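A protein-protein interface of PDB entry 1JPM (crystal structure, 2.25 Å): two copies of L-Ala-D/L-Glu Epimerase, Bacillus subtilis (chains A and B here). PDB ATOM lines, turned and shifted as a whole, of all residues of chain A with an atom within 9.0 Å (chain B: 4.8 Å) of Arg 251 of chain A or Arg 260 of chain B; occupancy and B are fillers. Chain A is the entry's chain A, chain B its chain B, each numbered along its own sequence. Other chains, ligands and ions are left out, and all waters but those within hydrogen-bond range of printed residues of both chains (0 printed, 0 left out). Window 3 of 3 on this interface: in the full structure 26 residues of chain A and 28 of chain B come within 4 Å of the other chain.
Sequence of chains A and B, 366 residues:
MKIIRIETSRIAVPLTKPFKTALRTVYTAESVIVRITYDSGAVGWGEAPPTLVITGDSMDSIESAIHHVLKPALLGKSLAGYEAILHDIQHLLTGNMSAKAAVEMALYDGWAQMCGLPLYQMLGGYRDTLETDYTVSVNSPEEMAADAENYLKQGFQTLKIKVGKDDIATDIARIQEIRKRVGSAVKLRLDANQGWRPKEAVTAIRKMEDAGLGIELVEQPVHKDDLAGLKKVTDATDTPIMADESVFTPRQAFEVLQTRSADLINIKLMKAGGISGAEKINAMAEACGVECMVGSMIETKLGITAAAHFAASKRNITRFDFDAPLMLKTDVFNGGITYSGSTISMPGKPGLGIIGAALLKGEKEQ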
ATOM      1  N   MET A  97     -35.700  33.986 -23.547  1.00  0.00           N
ATOM      2  CA  MET A  97     -36.209  34.278 -22.205  1.00  0.00           C
ATOM      3  C   MET A  97     -37.446  35.186 -22.166  1.00  0.00           C
ATOM      4  O   MET A  97     -38.321  35.005 -21.320  1.00  0.00           O
ATOM      5  CB  MET A  97     -35.104  34.893 -21.334  1.00  0.00           C
ATOM      6  CG  MET A  97     -33.843  34.046 -21.200  1.00  0.00           C
ATOM      7  SD  MET A  97     -34.122  32.349 -20.637  1.00  0.00           S
ATOM      8  CE  MET A  97     -33.979  32.552 -18.901  1.00  0.00           C
ATOM      9  N   LEU A 227     -17.263  38.626 -13.816  1.00  0.00           N
ATOM     10  CA  LEU A 227     -17.612  38.455 -12.415  1.00  0.00           C
ATOM     11  C   LEU A 227     -16.468  38.877 -11.497  1.00  0.00           C
ATOM     12  O   LEU A 227     -16.687  39.566 -10.496  1.00  0.00           O
ATOM     13  CB  LEU A 227     -17.991  36.997 -12.131  1.00  0.00           C
ATOM     14  CG  LEU A 227     -19.163  36.406 -12.928  1.00  0.00           C
ATOM     15  CD1 LEU A 227     -19.505  35.030 -12.371  1.00  0.00           C
ATOM     16  CD2 LEU A 227     -20.376  37.316 -12.848  1.00  0.00           C
ATOM     17  N   SER A 246     -25.395  40.685 -15.128  1.00  0.00           N
ATOM     18  CA  SER A 246     -24.555  39.539 -14.761  1.00  0.00           C
ATOM     19  C   SER A 246     -25.421  38.394 -14.247  1.00  0.00           C
ATOM     20  O   SER A 246     -24.958  37.259 -14.129  1.00  0.00           O
ATOM     21  CB  SER A 246     -23.538  39.908 -13.670  1.00  0.00           C
ATOM     22  OG  SER A 246     -22.385  40.522 -14.217  1.00  0.00           O
ATOM     23  N   VAL A 247     -26.675  38.693 -13.920  1.00  0.00           N
ATOM     24  CA  VAL A 247     -27.577  37.656 -13.429  1.00  0.00           C
ATOM     25  C   VAL A 247     -28.906  37.638 -14.160  1.00  0.00           C
ATOM     26  O   VAL A 247     -29.727  38.548 -13.995  1.00  0.00           O
ATOM     27  CB  VAL A 247     -27.885  37.810 -11.924  1.00  0.00           C
ATOM     28  CG1 VAL A 247     -28.881  36.739 -11.493  1.00  0.00           C
ATOM     29  CG2 VAL A 247     -26.608  37.693 -11.108  1.00  0.00           C
ATOM     30  N   PHE A 248     -29.107  36.600 -14.967  1.00  0.00           N
ATOM     31  CA  PHE A 248     -30.353  36.416 -15.702  1.00  0.00           C
ATOM     32  C   PHE A 248     -31.099  35.275 -15.048  1.00  0.00           C
ATOM     33  O   PHE A 248     -32.267  35.415 -14.681  1.00  0.00           O
ATOM     34  CB  PHE A 248     -30.106  36.025 -17.166  1.00  0.00           C
ATOM     35  CG  PHE A 248     -29.904  37.191 -18.097  1.00  0.00           C
ATOM     36  CD1 PHE A 248     -28.917  38.140 -17.854  1.00  0.00           C
ATOM     37  CD2 PHE A 248     -30.678  37.313 -19.250  1.00  0.00           C
ATOM     38  CE1 PHE A 248     -28.702  39.201 -18.754  1.00  0.00           C
ATOM     39  CE2 PHE A 248     -30.469  38.369 -20.156  1.00  0.00           C
ATOM     40  CZ  PHE A 248     -29.480  39.312 -19.904  1.00  0.00           C
ATOM     41  N   THR A 249     -30.394  34.156 -14.890  1.00  0.00           N
ATOM     42  CA  THR A 249     -30.945  32.920 -14.340  1.00  0.00           C
ATOM     43  C   THR A 249     -30.538  32.595 -12.901  1.00  0.00           C
ATOM     44  O   THR A 249     -29.621  33.193 -12.348  1.00  0.00           O
ATOM     45  CB  THR A 249     -30.502  31.715 -15.194  1.00  0.00           C
ATOM     46  OG1 THR A 249     -29.097  31.498 -14.992  1.00  0.00           O
ATOM     47  CG2 THR A 249     -30.753  31.972 -16.684  1.00  0.00           C
ATOM     48  N   PRO A 250     -31.221  31.623 -12.276  1.00  0.00           N
ATOM     49  CA  PRO A 250     -30.866  31.264 -10.900  1.00  0.00           C
ATOM     50  C   PRO A 250     -29.483  30.634 -10.799  1.00  0.00           C
ATOM     51  O   PRO A 250     -28.822  30.736  -9.766  1.00  0.00           O
ATOM     52  CB  PRO A 250     -31.994  30.317 -10.477  1.00  0.00           C
ATOM     53  CG  PRO A 250     -32.566  29.830 -11.756  1.00  0.00           C
ATOM     54  CD  PRO A 250     -32.512  31.023 -12.654  1.00  0.00           C
ATOM     55  N   ARG A 251     -29.043  29.985 -11.875  1.00  0.00           N
ATOM     56  CA  ARG A 251     -27.716  29.381 -11.886  1.00  0.00           C
ATOM     57  C   ARG A 251     -26.663  30.494 -11.863  1.00  0.00           C
ATOM     58  O   ARG A 251     -25.641  30.391 -11.188  1.00  0.00           O
ATOM     59  CB  ARG A 251     -27.545  28.513 -13.135  1.00  0.00           C
ATOM     60  CG  ARG A 251     -26.118  28.105 -13.443  1.00  0.00           C
ATOM     61  CD  ARG A 251     -25.482  27.317 -12.310  1.00  0.00           C
ATOM     62  NE  ARG A 251     -24.131  26.883 -12.660  1.00  0.00           N
ATOM     63  CZ  ARG A 251     -23.258  26.382 -11.793  1.00  0.00           C
ATOM     64  NH1 ARG A 251     -23.589  26.247 -10.514  1.00  0.00           N
ATOM     65  NH2 ARG A 251     -22.052  26.011 -12.208  1.00  0.00           N
ATOM     66  N   GLN A 252     -26.912  31.567 -12.602  1.00  0.00           N
ATOM     67  CA  GLN A 252     -25.968  32.671 -12.613  1.00  0.00           C
ATOM     68  C   GLN A 252     -26.031  33.402 -11.264  1.00  0.00           C
ATOM     69  O   GLN A 252     -25.033  33.947 -10.799  1.00  0.00           O
ATOM     70  CB  GLN A 252     -26.279  33.604 -13.781  1.00  0.00           C
ATOM     71  CG  GLN A 252     -26.222  32.873 -15.121  1.00  0.00           C
ATOM     72  CD  GLN A 252     -26.646  33.735 -16.295  1.00  0.00           C
ATOM     73  OE1 GLN A 252     -27.485  34.630 -16.159  1.00  0.00           O
ATOM     74  NE2 GLN A 252     -26.082  33.450 -17.469  1.00  0.00           N
ATOM     75  N   ALA A 253     -27.205  33.394 -10.636  1.00  0.00           N
ATOM     76  CA  ALA A 253     -27.380  34.029  -9.334  1.00  0.00           C
ATOM     77  C   ALA A 253     -26.511  33.265  -8.349  1.00  0.00           C
ATOM     78  O   ALA A 253     -25.762  33.850  -7.557  1.00  0.00           O
ATOM     79  CB  ALA A 253     -28.841  33.955  -8.898  1.00  0.00           C
ATOM     80  N   PHE A 254     -26.622  31.943  -8.416  1.00  0.00           N
ATOM     81  CA  PHE A 254     -25.867  31.056  -7.552  1.00  0.00           C
ATOM     82  C   PHE A 254     -24.360  31.337  -7.627  1.00  0.00           C
ATOM     83  O   PHE A 254     -23.679  31.374  -6.611  1.00  0.00           O
ATOM     84  CB  PHE A 254     -26.138  29.601  -7.947  1.00  0.00           C
ATOM     85  CG  PHE A 254     -25.624  28.614  -6.964  1.00  0.00           C
ATOM     86  CD1 PHE A 254     -26.444  28.143  -5.945  1.00  0.00           C
ATOM     87  CD2 PHE A 254     -24.299  28.173  -7.026  1.00  0.00           C
ATOM     88  CE1 PHE A 254     -25.959  27.248  -4.999  1.00  0.00           C
ATOM     89  CE2 PHE A 254     -23.803  27.278  -6.083  1.00  0.00           C
ATOM     90  CZ  PHE A 254     -24.634  26.814  -5.068  1.00  0.00           C
ATOM     91  N   GLU A 255     -23.853  31.526  -8.838  1.00  0.00           N
ATOM     92  CA  GLU A 255     -22.438  31.792  -9.066  1.00  0.00           C
ATOM     93  C   GLU A 255     -22.035  33.137  -8.456  1.00  0.00           C
ATOM     94  O   GLU A 255     -20.993  33.247  -7.803  1.00  0.00           O
ATOM     95  CB  GLU A 255     -22.165  31.775 -10.574  1.00  0.00           C
ATOM     96  CG  GLU A 255     -20.708  31.934 -10.989  1.00  0.00           C
ATOM     97  CD  GLU A 255     -19.806  30.848 -10.425  1.00  0.00           C
ATOM     98  OE1 GLU A 255     -20.229  29.670 -10.381  1.00  0.00           O
ATOM     99  OE2 GLU A 255     -18.663  31.173 -10.036  1.00  0.00           O
ATOM    100  N   VAL A 256     -22.865  34.156  -8.668  1.00  0.00           N
ATOM    101  CA  VAL A 256     -22.609  35.489  -8.125  1.00  0.00           C
ATOM    102  C   VAL A 256     -22.629  35.473  -6.598  1.00  0.00           C
ATOM    103  O   VAL A 256     -21.779  36.085  -5.956  1.00  0.00           O
ATOM    104  CB  VAL A 256     -23.659  36.508  -8.621  1.00  0.00           C
ATOM    105  CG1 VAL A 256     -23.583  37.792  -7.800  1.00  0.00           C
ATOM    106  CG2 VAL A 256     -23.417  36.818 -10.081  1.00  0.00           C
ATOM    107  N   LEU A 257     -23.603  34.774  -6.024  1.00  0.00           N
ATOM    108  CA  LEU A 257     -23.727  34.681  -4.569  1.00  0.00           C
ATOM    109  C   LEU A 257     -22.584  33.851  -3.988  1.00  0.00           C
ATOM    110  O   LEU A 257     -22.007  34.194  -2.949  1.00  0.00           O
ATOM    111  CB  LEU A 257     -25.064  34.033  -4.194  1.00  0.00           C
ATOM    112  CG  LEU A 257     -26.335  34.791  -4.590  1.00  0.00           C
ATOM    113  CD1 LEU A 257     -27.545  33.888  -4.353  1.00  0.00           C
ATOM    114  CD2 LEU A 257     -26.457  36.083  -3.785  1.00  0.00           C
ATOM    115  N   GLN A 258     -22.284  32.747  -4.669  1.00  0.00           N
ATOM    116  CA  GLN A 258     -21.225  31.824  -4.281  1.00  0.00           C
ATOM    117  C   GLN A 258     -19.875  32.545  -4.185  1.00  0.00           C
ATOM    118  O   GLN A 258     -19.113  32.333  -3.242  1.00  0.00           O
ATOM    119  CB  GLN A 258     -21.135  30.695  -5.315  1.00  0.00           C
ATOM    120  CG  GLN A 258     -19.936  29.788  -5.177  1.00  0.00           C
ATOM    121  CD  GLN A 258     -19.795  28.836  -6.357  1.00  0.00           C
ATOM    122  OE1 GLN A 258     -18.991  27.901  -6.321  1.00  0.00           O
ATOM    123  NE2 GLN A 258     -20.571  29.075  -7.414  1.00  0.00           N
ATOM    124  N   ILE A 265     -28.861  42.084  -6.028  1.00  0.00           N
ATOM    125  CA  ILE A 265     -29.196  41.520  -7.334  1.00  0.00           C
ATOM    126  C   ILE A 265     -30.479  42.167  -7.864  1.00  0.00           C
ATOM    127  O   ILE A 265     -31.457  42.304  -7.137  1.00  0.00           O
ATOM    128  CB  ILE A 265     -29.420  39.981  -7.252  1.00  0.00           C
ATOM    129  CG1 ILE A 265     -28.117  39.282  -6.868  1.00  0.00           C
ATOM    130  CG2 ILE A 265     -29.930  39.442  -8.597  1.00  0.00           C
ATOM    131  CD1 ILE A 265     -28.240  37.757  -6.779  1.00  0.00           C
ATOM    132  N   ALA A 272     -35.101  36.389 -16.507  1.00  0.00           N
ATOM    133  CA  ALA A 272     -35.285  35.095 -15.856  1.00  0.00           C
ATOM    134  C   ALA A 272     -36.220  34.149 -16.594  1.00  0.00           C
ATOM    135  O   ALA A 272     -36.391  32.995 -16.201  1.00  0.00           O
ATOM    136  CB  ALA A 272     -35.778  35.302 -14.434  1.00  0.00           C
ATOM    137  N   GLY A 277     -38.336  31.428 -12.345  1.00  0.00           N
ATOM    138  CA  GLY A 277     -36.905  31.648 -12.205  1.00  0.00           C
ATOM    139  C   GLY A 277     -36.607  32.812 -11.270  1.00  0.00           C
ATOM    140  O   GLY A 277     -35.656  32.759 -10.482  1.00  0.00           O
ATOM    141  N   LYS A 280     -36.715  31.687  -7.748  1.00  0.00           N
ATOM    142  CA  LYS A 280     -35.520  30.925  -7.399  1.00  0.00           C
ATOM    143  C   LYS A 280     -34.358  31.858  -7.062  1.00  0.00           C
ATOM    144  O   LYS A 280     -33.660  31.650  -6.070  1.00  0.00           O
ATOM    145  CB  LYS A 280     -35.118  29.990  -8.547  1.00  0.00           C
ATOM    146  CG  LYS A 280     -36.019  28.770  -8.703  1.00  0.00           C
ATOM    147  CD  LYS A 280     -35.440  27.796  -9.723  1.00  0.00           C
ATOM    148  CE  LYS A 280     -36.143  26.444  -9.674  1.00  0.00           C
ATOM    149  NZ  LYS A 280     -35.384  25.403 -10.434  1.00  0.00           N
ATOM    150  N   ILE A 281     -34.158  32.884  -7.887  1.00  0.00           N
ATOM    151  CA  ILE A 281     -33.083  33.841  -7.656  1.00  0.00           C
ATOM    152  C   ILE A 281     -33.234  34.501  -6.286  1.00  0.00           C
ATOM    153  O   ILE A 281     -32.301  34.501  -5.477  1.00  0.00           O
ATOM    154  CB  ILE A 281     -33.062  34.917  -8.765  1.00  0.00           C
ATOM    155  CG1 ILE A 281     -32.679  34.254 -10.094  1.00  0.00           C
ATOM    156  CG2 ILE A 281     -32.092  36.050  -8.396  1.00  0.00           C
ATOM    157  CD1 ILE A 281     -32.745  35.165 -11.282  1.00  0.00           C
ATOM    158  N   MET A 284     -32.481  32.097  -3.371  1.00  0.00           N
ATOM    159  CA  MET A 284     -31.055  31.829  -3.163  1.00  0.00           C
ATOM    160  C   MET A 284     -30.416  33.051  -2.512  1.00  0.00           C
ATOM    161  O   MET A 284     -29.630  32.932  -1.583  1.00  0.00           O
ATOM    162  CB  MET A 284     -30.323  31.592  -4.481  1.00  0.00           C
ATOM    163  CG  MET A 284     -30.879  30.512  -5.365  1.00  0.00           C
ATOM    164  SD  MET A 284     -29.853  30.358  -6.835  1.00  0.00           S
ATOM    165  CE  MET A 284     -30.014  28.587  -7.120  1.00  0.00           C
ATOM    166  N   LYS B 231     -17.024  15.599   1.157  1.00  0.00           N
ATOM    167  CA  LYS B 231     -16.571  15.849  -0.200  1.00  0.00           C
ATOM    168  C   LYS B 231     -15.480  14.865  -0.628  1.00  0.00           C
ATOM    169  O   LYS B 231     -15.393  14.492  -1.803  1.00  0.00           O
ATOM    170  CB  LYS B 231     -16.055  17.286  -0.339  1.00  0.00           C
ATOM    171  CG  LYS B 231     -15.590  17.602  -1.743  1.00  0.00           C
ATOM    172  CD  LYS B 231     -15.220  19.059  -1.923  1.00  0.00           C
ATOM    173  CE  LYS B 231     -14.899  19.323  -3.395  1.00  0.00           C
ATOM    174  NZ  LYS B 231     -14.646  20.766  -3.660  1.00  0.00           N
ATOM    175  N   THR B 234     -17.204  11.763  -1.690  1.00  0.00           N
ATOM    176  CA  THR B 234     -17.889  12.016  -2.953  1.00  0.00           C
ATOM    177  C   THR B 234     -16.908  11.961  -4.130  1.00  0.00           C
ATOM    178  O   THR B 234     -17.175  11.300  -5.132  1.00  0.00           O
ATOM    179  CB  THR B 234     -18.598  13.402  -2.929  1.00  0.00           C
ATOM    180  OG1 THR B 234     -19.642  13.389  -1.945  1.00  0.00           O
ATOM    181  CG2 THR B 234     -19.198  13.735  -4.297  1.00  0.00           C
ATOM    182  N   ASP B 235     -15.769  12.637  -3.998  1.00  0.00           N
ATOM    183  CA  ASP B 235     -14.770  12.678  -5.063  1.00  0.00           C
ATOM    184  C   ASP B 235     -13.872  11.450  -5.207  1.00  0.00           C
ATOM    185  O   ASP B 235     -13.169  11.318  -6.205  1.00  0.00           O
ATOM    186  CB  ASP B 235     -13.868  13.901  -4.900  1.00  0.00           C
ATOM    187  CG  ASP B 235     -14.618  15.205  -5.040  1.00  0.00           C
ATOM    188  OD1 ASP B 235     -15.733  15.189  -5.607  1.00  0.00           O
ATOM    189  OD2 ASP B 235     -14.084  16.247  -4.598  1.00  0.00           O
ATOM    190  N   VAL B 256     -23.294  23.009   0.804  1.00  0.00           N
ATOM    191  CA  VAL B 256     -23.002  21.694   0.250  1.00  0.00           C
ATOM    192  C   VAL B 256     -22.938  21.747  -1.278  1.00  0.00           C
ATOM    193  O   VAL B 256     -22.024  21.192  -1.886  1.00  0.00           O
ATOM    194  CB  VAL B 256     -24.068  20.665   0.700  1.00  0.00           C
ATOM    195  CG1 VAL B 256     -24.014  19.422  -0.176  1.00  0.00           C
ATOM    196  CG2 VAL B 256     -23.821  20.275   2.155  1.00  0.00           C
ATOM    197  N   LEU B 257     -23.889  22.437  -1.896  1.00  0.00           N
ATOM    198  CA  LEU B 257     -23.922  22.543  -3.357  1.00  0.00           C
ATOM    199  C   LEU B 257     -22.748  23.337  -3.914  1.00  0.00           C
ATOM    200  O   LEU B 257     -22.150  22.958  -4.920  1.00  0.00           O
ATOM    201  CB  LEU B 257     -25.228  23.196  -3.810  1.00  0.00           C
ATOM    202  CG  LEU B 257     -26.504  22.397  -3.548  1.00  0.00           C
ATOM    203  CD1 LEU B 257     -27.725  23.291  -3.773  1.00  0.00           C
ATOM    204  CD2 LEU B 257     -26.537  21.179  -4.462  1.00  0.00           C
ATOM    205  N   GLN B 258     -22.443  24.452  -3.260  1.00  0.00           N
ATOM    206  CA  GLN B 258     -21.350  25.328  -3.651  1.00  0.00           C
ATOM    207  C   GLN B 258     -19.994  24.616  -3.627  1.00  0.00           C
ATOM    208  O   GLN B 258     -19.171  24.795  -4.519  1.00  0.00           O
ATOM    209  CB  GLN B 258     -21.309  26.527  -2.704  1.00  0.00           C
ATOM    210  CG  GLN B 258     -19.922  27.094  -2.476  1.00  0.00           C
ATOM    211  CD  GLN B 258     -19.861  27.940  -1.235  1.00  0.00           C
ATOM    212  OE1 GLN B 258     -20.557  28.945  -1.122  1.00  0.00           O
ATOM    213  NE2 GLN B 258     -19.029  27.535  -0.284  1.00  0.00           N
ATOM    214  N   THR B 259     -19.764  23.821  -2.590  1.00  0.00           N
ATOM    215  CA  THR B 259     -18.510  23.095  -2.449  1.00  0.00           C
ATOM    216  C   THR B 259     -18.541  21.755  -3.196  1.00  0.00           C
ATOM    217  O   THR B 259     -17.525  21.079  -3.291  1.00  0.00           O
ATOM    218  CB  THR B 259     -18.206  22.824  -0.962  1.00  0.00           C
ATOM    219  OG1 THR B 259     -19.282  22.069  -0.390  1.00  0.00           O
ATOM    220  CG2 THR B 259     -18.058  24.131  -0.194  1.00  0.00           C
ATOM    221  N   ARG B 260     -19.710  21.388  -3.725  1.00  0.00           N
ATOM    222  CA  ARG B 260     -19.897  20.124  -4.446  1.00  0.00           C
ATOM    223  C   ARG B 260     -19.518  18.944  -3.560  1.00  0.00           C
ATOM    224  O   ARG B 260     -18.915  17.977  -4.022  1.00  0.00           O
ATOM    225  CB  ARG B 260     -19.049  20.096  -5.717  1.00  0.00           C
ATOM    226  CG  ARG B 260     -19.273  21.293  -6.613  1.00  0.00           C
ATOM    227  CD  ARG B 260     -19.221  20.888  -8.064  1.00  0.00           C
ATOM    228  NE  ARG B 260     -19.665  21.974  -8.928  1.00  0.00           N
ATOM    229  CZ  ARG B 260     -19.910  21.842 -10.227  1.00  0.00           C
ATOM    230  NH1 ARG B 260     -19.754  20.660 -10.814  1.00  0.00           N
ATOM    231  NH2 ARG B 260     -20.312  22.890 -10.933  1.00  0.00           N
ATOM    232  N   SER B 261     -19.894  19.030  -2.289  1.00  0.00           N
ATOM    233  CA  SER B 261     -19.571  18.001  -1.307  1.00  0.00           C
ATOM    234  C   SER B 261     -20.447  16.756  -1.333  1.00  0.00           C
ATOM    235  O   SER B 261     -20.197  15.815  -0.588  1.00  0.00           O
ATOM    236  CB  SER B 261     -19.605  18.608   0.098  1.00  0.00           C
ATOM    237  OG  SER B 261     -18.723  19.716   0.196  1.00  0.00           O
ATOM    238  N   ALA B 262     -21.471  16.744  -2.177  1.00  0.00           N
ATOM    239  CA  ALA B 262     -22.354  15.584  -2.263  1.00  0.00           C
ATOM    240  C   ALA B 262     -23.054  15.519  -3.613  1.00  0.00           C
ATOM    241  O   ALA B 262     -23.282  16.547  -4.261  1.00  0.00           O
ATOM    242  CB  ALA B 262     -23.388  15.616  -1.139  1.00  0.00           C
ATOM    243  N   ALA B 287     -31.315  23.697  -9.546  1.00  0.00           N
ATOM    244  CA  ALA B 287     -30.554  24.652 -10.346  1.00  0.00           C
ATOM    245  C   ALA B 287     -29.083  24.240 -10.477  1.00  0.00           C
ATOM    246  O   ALA B 287     -28.373  24.724 -11.362  1.00  0.00           O
ATOM    247  CB  ALA B 287     -30.653  26.047  -9.722  1.00  0.00           C
ATOM    248  N   CYS B 288     -28.625  23.365  -9.582  1.00  0.00           N
ATOM    249  CA  CYS B 288     -27.246  22.886  -9.618  1.00  0.00           C
ATOM    250  C   CYS B 288     -27.180  21.471 -10.196  1.00  0.00           C
ATOM    251  O   CYS B 288     -26.125  20.838 -10.195  1.00  0.00           O
ATOM    252  CB  CYS B 288     -26.634  22.896  -8.215  1.00  0.00           C
ATOM    253  SG  CYS B 288     -26.472  24.547  -7.493  1.00  0.00           S
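Ser 246 of chain A touches none of the printed residues of chain B. Val 247 of chain A touches none of the printed residues of chain B. Printed residues of chain B within 4 Å of Arg 251 of chain A: Arg 260 (3.8 Å) and Ala 287 (3.998 Å). Printed residues of chain A within 4 Å of Gln 258 of chain B: Phe 254 (3.7 Å) and Gln 258 (3.6 Å). No residue of chain A comes within 4 Å of Thr 259 of chain B. Of chain A, only Arg 251 (3.8 Å) comes within 4 Å of Arg 260 of chain B. Ser 261 of chain B touches none of the printed residues of chain A. Printed residues of chain A within 4 Å of Ala 287 of chain B: Arg 251 and Met 284. Printed residues of chain A within 4 Å of Cys 288 of chain B: Phe 254 (3.7 Å). The nearest residue of chain A that does not touch Arg 260 of chain B is Gln 258 of chain A (6.5 Å).
NH2 of Arg 260 of chain B touches NH2 of Arg 251 of chain A, 3.8 Å away. CD of Arg 251 of chain A touches O of Ala 287 of chain B, 3.998 Å away. Phe 254 of chain A touches Leu 257 of chain B. Phe 254 of chain A touches Gln 258 of chain B (CZ to N, 3.7 Å). Phe 254 of chain A touches Cys 288 of chain B (CE1 to SG, 3.7 Å). Gln 258 of chain A touches Gln 258 of chain B (OE1 to O, 3.6 Å). Ala 287 of chain B touches Met 284 of chain A (CB to CE, 3.7 Å).
Of the 21 printed residues of chain A, 4 touch a printed residue of chain B. Hydrophobic or aromatic side chains of chain A within 4 Å of the printed part of chain B: Phe 254 and Met 284. Of the 12 printed residues of chain B, 5 touch a printed residue of chain A.
Gln 258 of chain B touches its own counterpart, Gln 258 of chain A. Positions printed for both chains: 256, 257 and 258.
The side-chain amide nitrogen (NE2) of Gln 258 of chain A lies within hydrogen-bond range of the side-chain carboxylate (OE1) of Glu 255 of chain A, at 3.0 Å. OG1 of Thr 249 of chain A lies close to N of Arg 251 of chain A, 3.5 Å away.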
